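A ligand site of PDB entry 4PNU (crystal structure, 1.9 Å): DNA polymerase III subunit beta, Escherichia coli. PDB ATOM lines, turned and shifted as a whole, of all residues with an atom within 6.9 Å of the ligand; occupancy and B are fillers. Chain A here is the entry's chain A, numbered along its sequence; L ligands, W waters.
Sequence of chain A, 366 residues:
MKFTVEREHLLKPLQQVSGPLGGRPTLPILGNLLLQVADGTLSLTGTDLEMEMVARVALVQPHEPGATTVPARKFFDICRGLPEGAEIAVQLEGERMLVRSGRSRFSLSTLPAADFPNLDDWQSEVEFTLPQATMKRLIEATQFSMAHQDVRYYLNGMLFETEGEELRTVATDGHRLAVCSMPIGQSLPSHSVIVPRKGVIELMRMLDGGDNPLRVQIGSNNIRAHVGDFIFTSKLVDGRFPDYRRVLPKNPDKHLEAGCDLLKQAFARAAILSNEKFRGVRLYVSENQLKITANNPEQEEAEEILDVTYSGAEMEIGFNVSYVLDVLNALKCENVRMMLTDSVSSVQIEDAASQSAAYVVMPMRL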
ATOM      1  N   ASP A 150      -3.004  23.378 -16.045  1.00  0.00           N
ATOM      2  CA  ASP A 150      -2.320  22.128 -16.357  1.00  0.00           C
ATOM      3  C   ASP A 150      -2.997  21.462 -17.543  1.00  0.00           C
ATOM      4  O   ASP A 150      -4.238  21.504 -17.666  1.00  0.00           O
ATOM      5  CB  ASP A 150      -2.351  21.179 -15.152  1.00  0.00           C
ATOM      6  CG  ASP A 150      -1.224  20.149 -15.183  1.00  0.00           C
ATOM      7  OD1 ASP A 150      -1.314  19.161 -15.939  1.00  0.00           O
ATOM      8  OD2 ASP A 150      -0.244  20.315 -14.428  1.00  0.00           O
ATOM      9  N   ARG A 152      -3.354  18.455 -17.781  1.00  0.00           N
ATOM     10  CA  ARG A 152      -4.241  17.510 -17.128  1.00  0.00           C
ATOM     11  C   ARG A 152      -5.419  18.302 -16.590  1.00  0.00           C
ATOM     12  O   ARG A 152      -5.386  18.820 -15.468  1.00  0.00           O
ATOM     13  CB  ARG A 152      -3.514  16.760 -16.017  1.00  0.00           C
ATOM     14  CG  ARG A 152      -2.439  15.833 -16.536  1.00  0.00           C
ATOM     15  CD  ARG A 152      -1.445  15.460 -15.438  1.00  0.00           C
ATOM     16  NE  ARG A 152      -0.757  16.621 -14.888  1.00  0.00           N
ATOM     17  CZ  ARG A 152       0.194  16.567 -13.961  1.00  0.00           C
ATOM     18  NH1 ARG A 152       0.611  15.409 -13.475  1.00  0.00           N
ATOM     19  NH2 ARG A 152       0.753  17.695 -13.534  1.00  0.00           N
ATOM     20  N   TYR A 154      -8.289  17.672 -15.517  1.00  0.00           N
ATOM     21  CA  TYR A 154      -8.938  17.179 -14.298  1.00  0.00           C
ATOM     22  C   TYR A 154      -8.330  17.733 -12.993  1.00  0.00           C
ATOM     23  O   TYR A 154      -8.976  17.665 -11.946  1.00  0.00           O
ATOM     24  CB  TYR A 154      -8.965  15.655 -14.276  1.00  0.00           C
ATOM     25  CG  TYR A 154      -7.619  14.958 -14.362  1.00  0.00           C
ATOM     26  CD1 TYR A 154      -6.841  14.758 -13.238  1.00  0.00           C
ATOM     27  CD2 TYR A 154      -7.152  14.460 -15.587  1.00  0.00           C
ATOM     28  CE1 TYR A 154      -5.609  14.091 -13.312  1.00  0.00           C
ATOM     29  CE2 TYR A 154      -5.923  13.802 -15.672  1.00  0.00           C
ATOM     30  CZ  TYR A 154      -5.160  13.619 -14.531  1.00  0.00           C
ATOM     31  OH  TYR A 154      -3.936  12.969 -14.618  1.00  0.00           O
ATOM     32  N   LEU A 155      -7.117  18.266 -13.084  1.00  0.00           N
ATOM     33  CA  LEU A 155      -6.438  18.903 -11.938  1.00  0.00           C
ATOM     34  C   LEU A 155      -6.717  20.385 -11.809  1.00  0.00           C
ATOM     35  O   LEU A 155      -6.334  20.975 -10.797  1.00  0.00           O
ATOM     36  CB  LEU A 155      -4.906  18.722 -12.040  1.00  0.00           C
ATOM     37  CG  LEU A 155      -4.328  17.324 -12.035  1.00  0.00           C
ATOM     38  CD1 LEU A 155      -2.816  17.386 -12.063  1.00  0.00           C
ATOM     39  CD2 LEU A 155      -4.801  16.535 -10.819  1.00  0.00           C
ATOM     40  N   THR A 172      -5.069  19.043  -6.089  1.00  0.00           N
ATOM     41  CA  THR A 172      -3.665  18.792  -6.334  1.00  0.00           C
ATOM     42  C   THR A 172      -3.242  19.322  -7.692  1.00  0.00           C
ATOM     43  O   THR A 172      -4.055  19.442  -8.617  1.00  0.00           O
ATOM     44  CB  THR A 172      -3.333  17.291  -6.182  1.00  0.00           C
ATOM     45  OG1 THR A 172      -1.914  17.089  -6.311  1.00  0.00           O
ATOM     46  CG2 THR A 172      -4.040  16.472  -7.208  1.00  0.00           C
ATOM     47  N   ASP A 173      -1.965  19.669  -7.794  1.00  0.00           N
ATOM     48  CA  ASP A 173      -1.406  20.152  -9.056  1.00  0.00           C
ATOM     49  C   ASP A 173      -0.277  19.260  -9.542  1.00  0.00           C
ATOM     50  O   ASP A 173       0.428  19.622 -10.467  1.00  0.00           O
ATOM     51  CB  ASP A 173      -0.953  21.614  -8.920  1.00  0.00           C
ATOM     52  CG  ASP A 173       0.201  21.797  -7.936  1.00  0.00           C
ATOM     53  OD1 ASP A 173       0.737  20.795  -7.393  1.00  0.00           O
ATOM     54  OD2 ASP A 173       0.560  22.980  -7.705  1.00  0.00           O
ATOM     55  N   GLY A 174      -0.131  18.073  -8.938  1.00  0.00           N
ATOM     56  CA  GLY A 174       0.938  17.147  -9.284  1.00  0.00           C
ATOM     57  C   GLY A 174       2.191  17.250  -8.419  1.00  0.00           C
ATOM     58  O   GLY A 174       2.997  16.309  -8.367  1.00  0.00           O
ATOM     59  N   HIS A 175       2.361  18.397  -7.749  1.00  0.00           N
ATOM     60  CA  HIS A 175       3.550  18.644  -6.924  1.00  0.00           C
ATOM     61  C   HIS A 175       3.205  18.695  -5.444  1.00  0.00           C
ATOM     62  O   HIS A 175       4.040  18.382  -4.582  1.00  0.00           O
ATOM     63  CB  HIS A 175       4.200  19.955  -7.343  1.00  0.00           C
ATOM     64  CG  HIS A 175       4.526  20.047  -8.800  1.00  0.00           C
ATOM     65  ND1 HIS A 175       3.647  20.580  -9.728  1.00  0.00           N
ATOM     66  CD2 HIS A 175       5.625  19.694  -9.500  1.00  0.00           C
ATOM     67  CE1 HIS A 175       4.206  20.554 -10.919  1.00  0.00           C
ATOM     68  NE2 HIS A 175       5.406  20.025 -10.807  1.00  0.00           N
ATOM     69  N   ARG A 176       1.983  19.136  -5.147  1.00  0.00           N
ATOM     70  CA  ARG A 176       1.473  19.179  -3.801  1.00  0.00           C
ATOM     71  C   ARG A 176      -0.030  18.902  -3.776  1.00  0.00           C
ATOM     72  O   ARG A 176      -0.723  19.075  -4.786  1.00  0.00           O
ATOM     73  CB  ARG A 176       1.821  20.519  -3.111  1.00  0.00           C
ATOM     74  CG  ARG A 176       1.761  21.770  -3.984  1.00  0.00           C
ATOM     75  CD  ARG A 176       0.348  22.298  -4.148  1.00  0.00           C
ATOM     76  NE  ARG A 176       0.308  23.511  -4.964  1.00  0.00           N
ATOM     77  CZ  ARG A 176       0.575  24.745  -4.519  1.00  0.00           C
ATOM     78  NH1 ARG A 176       0.917  24.983  -3.254  1.00  0.00           N
ATOM     79  NH2 ARG A 176       0.486  25.753  -5.364  1.00  0.00           N
ATOM     80  N   LEU A 177      -0.519  18.451  -2.632  1.00  0.00           N
ATOM     81  CA  LEU A 177      -1.921  18.076  -2.488  1.00  0.00           C
ATOM     82  C   LEU A 177      -2.484  18.581  -1.174  1.00  0.00           C
ATOM     83  O   LEU A 177      -1.771  18.652  -0.153  1.00  0.00           O
ATOM     84  CB  LEU A 177      -2.076  16.541  -2.601  1.00  0.00           C
ATOM     85  CG  LEU A 177      -3.451  15.911  -2.332  1.00  0.00           C
ATOM     86  CD1 LEU A 177      -3.675  14.679  -3.209  1.00  0.00           C
ATOM     87  CD2 LEU A 177      -3.658  15.553  -0.862  1.00  0.00           C
ATOM     88  N   ALA A 178      -3.761  18.928  -1.208  1.00  0.00           N
ATOM     89  CA  ALA A 178      -4.526  19.230  -0.033  1.00  0.00           C
ATOM     90  C   ALA A 178      -5.808  18.377  -0.046  1.00  0.00           C
ATOM     91  O   ALA A 178      -6.441  18.197  -1.086  1.00  0.00           O
ATOM     92  CB  ALA A 178      -4.868  20.696  -0.001  1.00  0.00           C
ATOM     93  N   ARG A 240     -10.021  11.116 -14.741  1.00  0.00           N
ATOM     94  CA  ARG A 240      -9.837  10.309 -13.547  1.00  0.00           C
ATOM     95  C   ARG A 240      -8.966  11.064 -12.552  1.00  0.00           C
ATOM     96  O   ARG A 240      -7.751  11.137 -12.705  1.00  0.00           O
ATOM     97  CB  ARG A 240      -9.195   8.961 -13.888  1.00  0.00           C
ATOM     98  CG  ARG A 240     -10.090   8.005 -14.679  1.00  0.00           C
ATOM     99  CD  ARG A 240      -9.638   6.546 -14.540  1.00  0.00           C
ATOM    100  NE  ARG A 240      -8.203   6.402 -14.728  1.00  0.00           N
ATOM    101  CZ  ARG A 240      -7.574   6.465 -15.892  1.00  0.00           C
ATOM    102  NH1 ARG A 240      -8.261   6.657 -17.024  1.00  0.00           N
ATOM    103  NH2 ARG A 240      -6.247   6.329 -15.942  1.00  0.00           N
ATOM    104  N   PHE A 241      -9.589  11.628 -11.532  1.00  0.00           N
ATOM    105  CA  PHE A 241      -8.859  12.345 -10.499  1.00  0.00           C
ATOM    106  C   PHE A 241      -7.961  11.360  -9.722  1.00  0.00           C
ATOM    107  O   PHE A 241      -8.335  10.199  -9.545  1.00  0.00           O
ATOM    108  CB  PHE A 241      -9.819  13.068  -9.555  1.00  0.00           C
ATOM    109  CG  PHE A 241      -9.191  14.222  -8.834  1.00  0.00           C
ATOM    110  CD1 PHE A 241      -9.118  15.461  -9.436  1.00  0.00           C
ATOM    111  CD2 PHE A 241      -8.663  14.067  -7.566  1.00  0.00           C
ATOM    112  CE1 PHE A 241      -8.537  16.544  -8.787  1.00  0.00           C
ATOM    113  CE2 PHE A 241      -8.064  15.137  -6.913  1.00  0.00           C
ATOM    114  CZ  PHE A 241      -8.011  16.366  -7.510  1.00  0.00           C
ATOM    115  N   PRO A 242      -6.784  11.819  -9.274  1.00  0.00           N
ATOM    116  CA  PRO A 242      -5.953  10.908  -8.453  1.00  0.00           C
ATOM    117  C   PRO A 242      -6.592  10.554  -7.121  1.00  0.00           C
ATOM    118  O   PRO A 242      -7.486  11.251  -6.645  1.00  0.00           O
ATOM    119  CB  PRO A 242      -4.658  11.725  -8.199  1.00  0.00           C
ATOM    120  CG  PRO A 242      -5.021  13.138  -8.501  1.00  0.00           C
ATOM    121  CD  PRO A 242      -6.072  13.079  -9.575  1.00  0.00           C
ATOM    122  N   VAL A 247      -1.467   9.320  -2.428  1.00  0.00           N
ATOM    123  CA  VAL A 247      -0.586  10.464  -2.303  1.00  0.00           C
ATOM    124  C   VAL A 247      -0.135  10.607  -0.854  1.00  0.00           C
ATOM    125  O   VAL A 247       1.014  10.927  -0.596  1.00  0.00           O
ATOM    126  CB  VAL A 247      -1.270  11.752  -2.785  1.00  0.00           C
ATOM    127  CG1 VAL A 247      -0.356  12.959  -2.602  1.00  0.00           C
ATOM    128  CG2 VAL A 247      -1.699  11.620  -4.249  1.00  0.00           C
ATOM    129  N   SER A 346       7.465  11.964   0.025  1.00  0.00           N
ATOM    130  CA  SER A 346       6.660  13.128   0.360  1.00  0.00           C
ATOM    131  C   SER A 346       6.551  13.328   1.875  1.00  0.00           C
ATOM    132  O   SER A 346       6.751  12.404   2.642  1.00  0.00           O
ATOM    133  CB  SER A 346       5.262  12.985  -0.242  1.00  0.00           C
ATOM    134  OG  SER A 346       4.577  11.907   0.392  1.00  0.00           O
ATOM    135  N   VAL A 347       6.177  14.544   2.264  1.00  0.00           N
ATOM    136  CA  VAL A 347       5.919  14.847   3.647  1.00  0.00           C
ATOM    137  C   VAL A 347       4.477  15.251   3.818  1.00  0.00           C
ATOM    138  O   VAL A 347       3.910  15.932   2.954  1.00  0.00           O
ATOM    139  CB  VAL A 347       6.838  15.973   4.112  1.00  0.00           C
ATOM    140  CG1 VAL A 347       6.433  16.493   5.475  1.00  0.00           C
ATOM    141  CG2 VAL A 347       8.254  15.430   4.102  1.00  0.00           C
ATOM    142  N   TYR A 359      -2.055  17.821   4.181  1.00  0.00           N
ATOM    143  CA  TYR A 359      -1.332  18.420   3.082  1.00  0.00           C
ATOM    144  C   TYR A 359      -0.139  17.547   2.786  1.00  0.00           C
ATOM    145  O   TYR A 359       0.550  17.094   3.717  1.00  0.00           O
ATOM    146  CB  TYR A 359      -0.875  19.833   3.478  1.00  0.00           C
ATOM    147  CG  TYR A 359      -2.078  20.693   3.802  1.00  0.00           C
ATOM    148  CD1 TYR A 359      -2.780  21.336   2.802  1.00  0.00           C
ATOM    149  CD2 TYR A 359      -2.557  20.781   5.104  1.00  0.00           C
ATOM    150  CE1 TYR A 359      -3.912  22.077   3.074  1.00  0.00           C
ATOM    151  CE2 TYR A 359      -3.692  21.522   5.386  1.00  0.00           C
ATOM    152  CZ  TYR A 359      -4.372  22.175   4.370  1.00  0.00           C
ATOM    153  OH  TYR A 359      -5.496  22.921   4.645  1.00  0.00           O
ATOM    154  N   VAL A 360       0.110  17.300   1.502  1.00  0.00           N
ATOM    155  CA  VAL A 360       1.256  16.510   1.090  1.00  0.00           C
ATOM    156  C   VAL A 360       2.076  17.306   0.094  1.00  0.00           C
ATOM    157  O   VAL A 360       1.537  17.910  -0.845  1.00  0.00           O
ATOM    158  CB  VAL A 360       0.846  15.169   0.468  1.00  0.00           C
ATOM    159  CG1 VAL A 360       2.081  14.321   0.182  1.00  0.00           C
ATOM    160  CG2 VAL A 360      -0.111  14.435   1.388  1.00  0.00           C
ATOM    161  N   VAL A 361       3.387  17.307   0.315  1.00  0.00           N
ATOM    162  CA  VAL A 361       4.318  18.052  -0.519  1.00  0.00           C
ATOM    163  C   VAL A 361       5.441  17.116  -0.965  1.00  0.00           C
ATOM    164  O   VAL A 361       6.040  16.421  -0.154  1.00  0.00           O
ATOM    165  CB  VAL A 361       4.882  19.272   0.257  1.00  0.00           C
ATOM    166  CG1 VAL A 361       5.926  20.023  -0.570  1.00  0.00           C
ATOM    167  CG2 VAL A 361       3.758  20.202   0.672  1.00  0.00           C
ATOM    168  N   MET A 362       5.693  17.088  -2.262  1.00  0.00           N
ATOM    169  CA  MET A 362       6.721  16.212  -2.805  1.00  0.00           C
ATOM    170  C   MET A 362       8.116  16.733  -2.438  1.00  0.00           C
ATOM    171  O   MET A 362       8.318  17.937  -2.246  1.00  0.00           O
ATOM    172  CB  MET A 362       6.532  16.054  -4.322  1.00  0.00           C
ATOM    173  CG  MET A 362       6.734  14.650  -4.864  1.00  0.00           C
ATOM    174  SD  MET A 362       6.153  13.234  -3.879  1.00  0.00           S
ATOM    175  CE  MET A 362       7.343  11.980  -4.313  1.00  0.00           C
ATOM    176  N   PRO A 363       9.079  15.812  -2.296  1.00  0.00           N
ATOM    177  CA  PRO A 363      10.368  16.324  -1.904  1.00  0.00           C
ATOM    178  C   PRO A 363      11.104  16.816  -3.142  1.00  0.00           C
ATOM    179  O   PRO A 363      10.715  16.504  -4.273  1.00  0.00           O
ATOM    180  CB  PRO A 363      11.044  15.098  -1.291  1.00  0.00           C
ATOM    181  CG  PRO A 363      10.484  13.950  -2.067  1.00  0.00           C
ATOM    182  CD  PRO A 363       9.137  14.376  -2.605  1.00  0.00           C
HETATM  183  C1  LIG L   1      -1.228  14.148  -8.508  1.00  0.00           C
HETATM  184  C2  LIG L   1      -1.521  14.170  -9.982  1.00  0.00           C
HETATM  185  C3  LIG L   1      -1.200  12.832 -10.599  1.00  0.00           C
HETATM  186  C4  LIG L   1      -1.712  12.789 -12.085  1.00  0.00           C
HETATM  187  O1  LIG L   1      -2.931  12.526 -12.238  1.00  0.00           O
HETATM  188  O2  LIG L   1      -0.908  12.972 -13.033  1.00  0.00           O
HETATM  189  C5  LIG L   1       0.274  12.591 -10.507  1.00  0.00           C
HETATM  190  C6  LIG L   1       0.793  13.040  -9.264  1.00  0.00           C
HETATM  191  C7  LIG L   1       0.114  13.755  -8.333  1.00  0.00           C
HETATM  192  C8  LIG L   1       0.942  13.976  -7.276  1.00  0.00           C
HETATM  193  C9  LIG L   1       0.780  14.645  -6.113  1.00  0.00           C
HETATM  194  C10 LIG L   1       1.827  14.727  -5.175  1.00  0.00           C
HETATM  195 BR1  LIG L   1       1.705  15.642  -3.543  1.00  0.00          BR
HETATM  196  C11 LIG L   1       3.034  14.114  -5.483  1.00  0.00           C
HETATM  197  C12 LIG L   1       3.157  13.450  -6.697  1.00  0.00           C
HETATM  198  C13 LIG L   1       2.128  13.390  -7.559  1.00  0.00           C
HETATM  199  N1  LIG L   1       2.020  12.830  -8.760  1.00  0.00           N
HETATM  200  C14 LIG L   1       3.105  12.077  -9.456  1.00  0.00           C
HETATM  201  C15 LIG L   1       3.989  12.956 -10.376  1.00  0.00           C
HETATM  202  O3  LIG L   1       4.759  12.407 -11.154  1.00  0.00           O
HETATM  203  N2  LIG L   1       3.930  14.300 -10.282  1.00  0.00           N
HETATM  204  C16 LIG L   1       4.768  15.150 -11.142  1.00  0.00           C
HETATM  205  C17 LIG L   1       3.932  16.136 -11.985  1.00  0.00           C
HETATM  206  O4  LIG L   1       2.709  16.194 -11.774  1.00  0.00           O
HETATM  207  O5  LIG L   1       4.565  16.820 -12.810  1.00  0.00           O
HETATM  208  C18 LIG L   1       5.771  15.935 -10.279  1.00  0.00           C
HETATM  209  C19 LIG L   1       6.581  14.953  -9.689  1.00  0.00           C
HETATM  210  C20 LIG L   1       7.651  14.418 -10.413  1.00  0.00           C
HETATM  211  C21 LIG L   1       8.459  13.431  -9.855  1.00  0.00           C
HETATM  212  C22 LIG L   1       8.208  12.961  -8.568  1.00  0.00           C
HETATM  213  C23 LIG L   1       7.139  13.474  -7.843  1.00  0.00           C
HETATM  214  C24 LIG L   1       6.319  14.479  -8.395  1.00  0.00           C
HETATM  215  O   HOH W   1       1.719  11.575 -13.870  1.00  0.00           O
HETATM  216  O   HOH W   2       0.654  10.057  -7.171  1.00  0.00           O
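The side-chain hydroxyl (OH) of Tyr 154 sits at hydrogen-bond distance from an oxygen (O1) of the ligand (2.6 Å).
The guanidinium group of Arg 152 lies within salt-bridge range of an oxygen (O4) of the ligand (2.8 Å).
O of Gly 174 lies within hydrogen-bond range of N2 of the ligand, 2.9 Å away.
Merely in contact with the ligand: Met 362, Val 247, Val 360, Arg 176, Thr 172, Leu 177, His 175 and Pro 242.
Hydrophobic or aromatic side chains within 4 Å of the ligand: Tyr 154, His 175, Leu 177, Pro 242, Val 247, Val 360 and Met 362.
Of the 22 residues printed, 11 come within 4 Å of the ligand.
The nearest printed residue that does not touch the ligand is Leu 155 (4.04 Å).
The backbone NH (N) of Gly 174 is in hydrogen-bond range of the side-chain hydroxyl (OG1) of Thr 172 (3.3 Å).
The backbone NH of His 175 is in hydrogen-bond range of the side-chain carboxylate of Asp 173, 2.9 Å away.
The side-chain hydroxyl (OG1) of Thr 172 is in hydrogen-bond range of the backbone carbonyl oxygen (O) of Arg 176.
The guanidinium group (NE) of Arg 176 is in salt-bridge range of the side-chain carboxylate (OD2) of Asp 173.
O of Val 360 sits at hydrogen-bond distance from N of Leu 177 (2.8 Å).
The side-chain carboxylate (OD1) of Asp 150 lies within salt-bridge range of the guanidinium group (NE) of Arg 152, at 2.8 Å.
N of Met 362 is in hydrogen-bond range of O of His 175 (3.1 Å).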
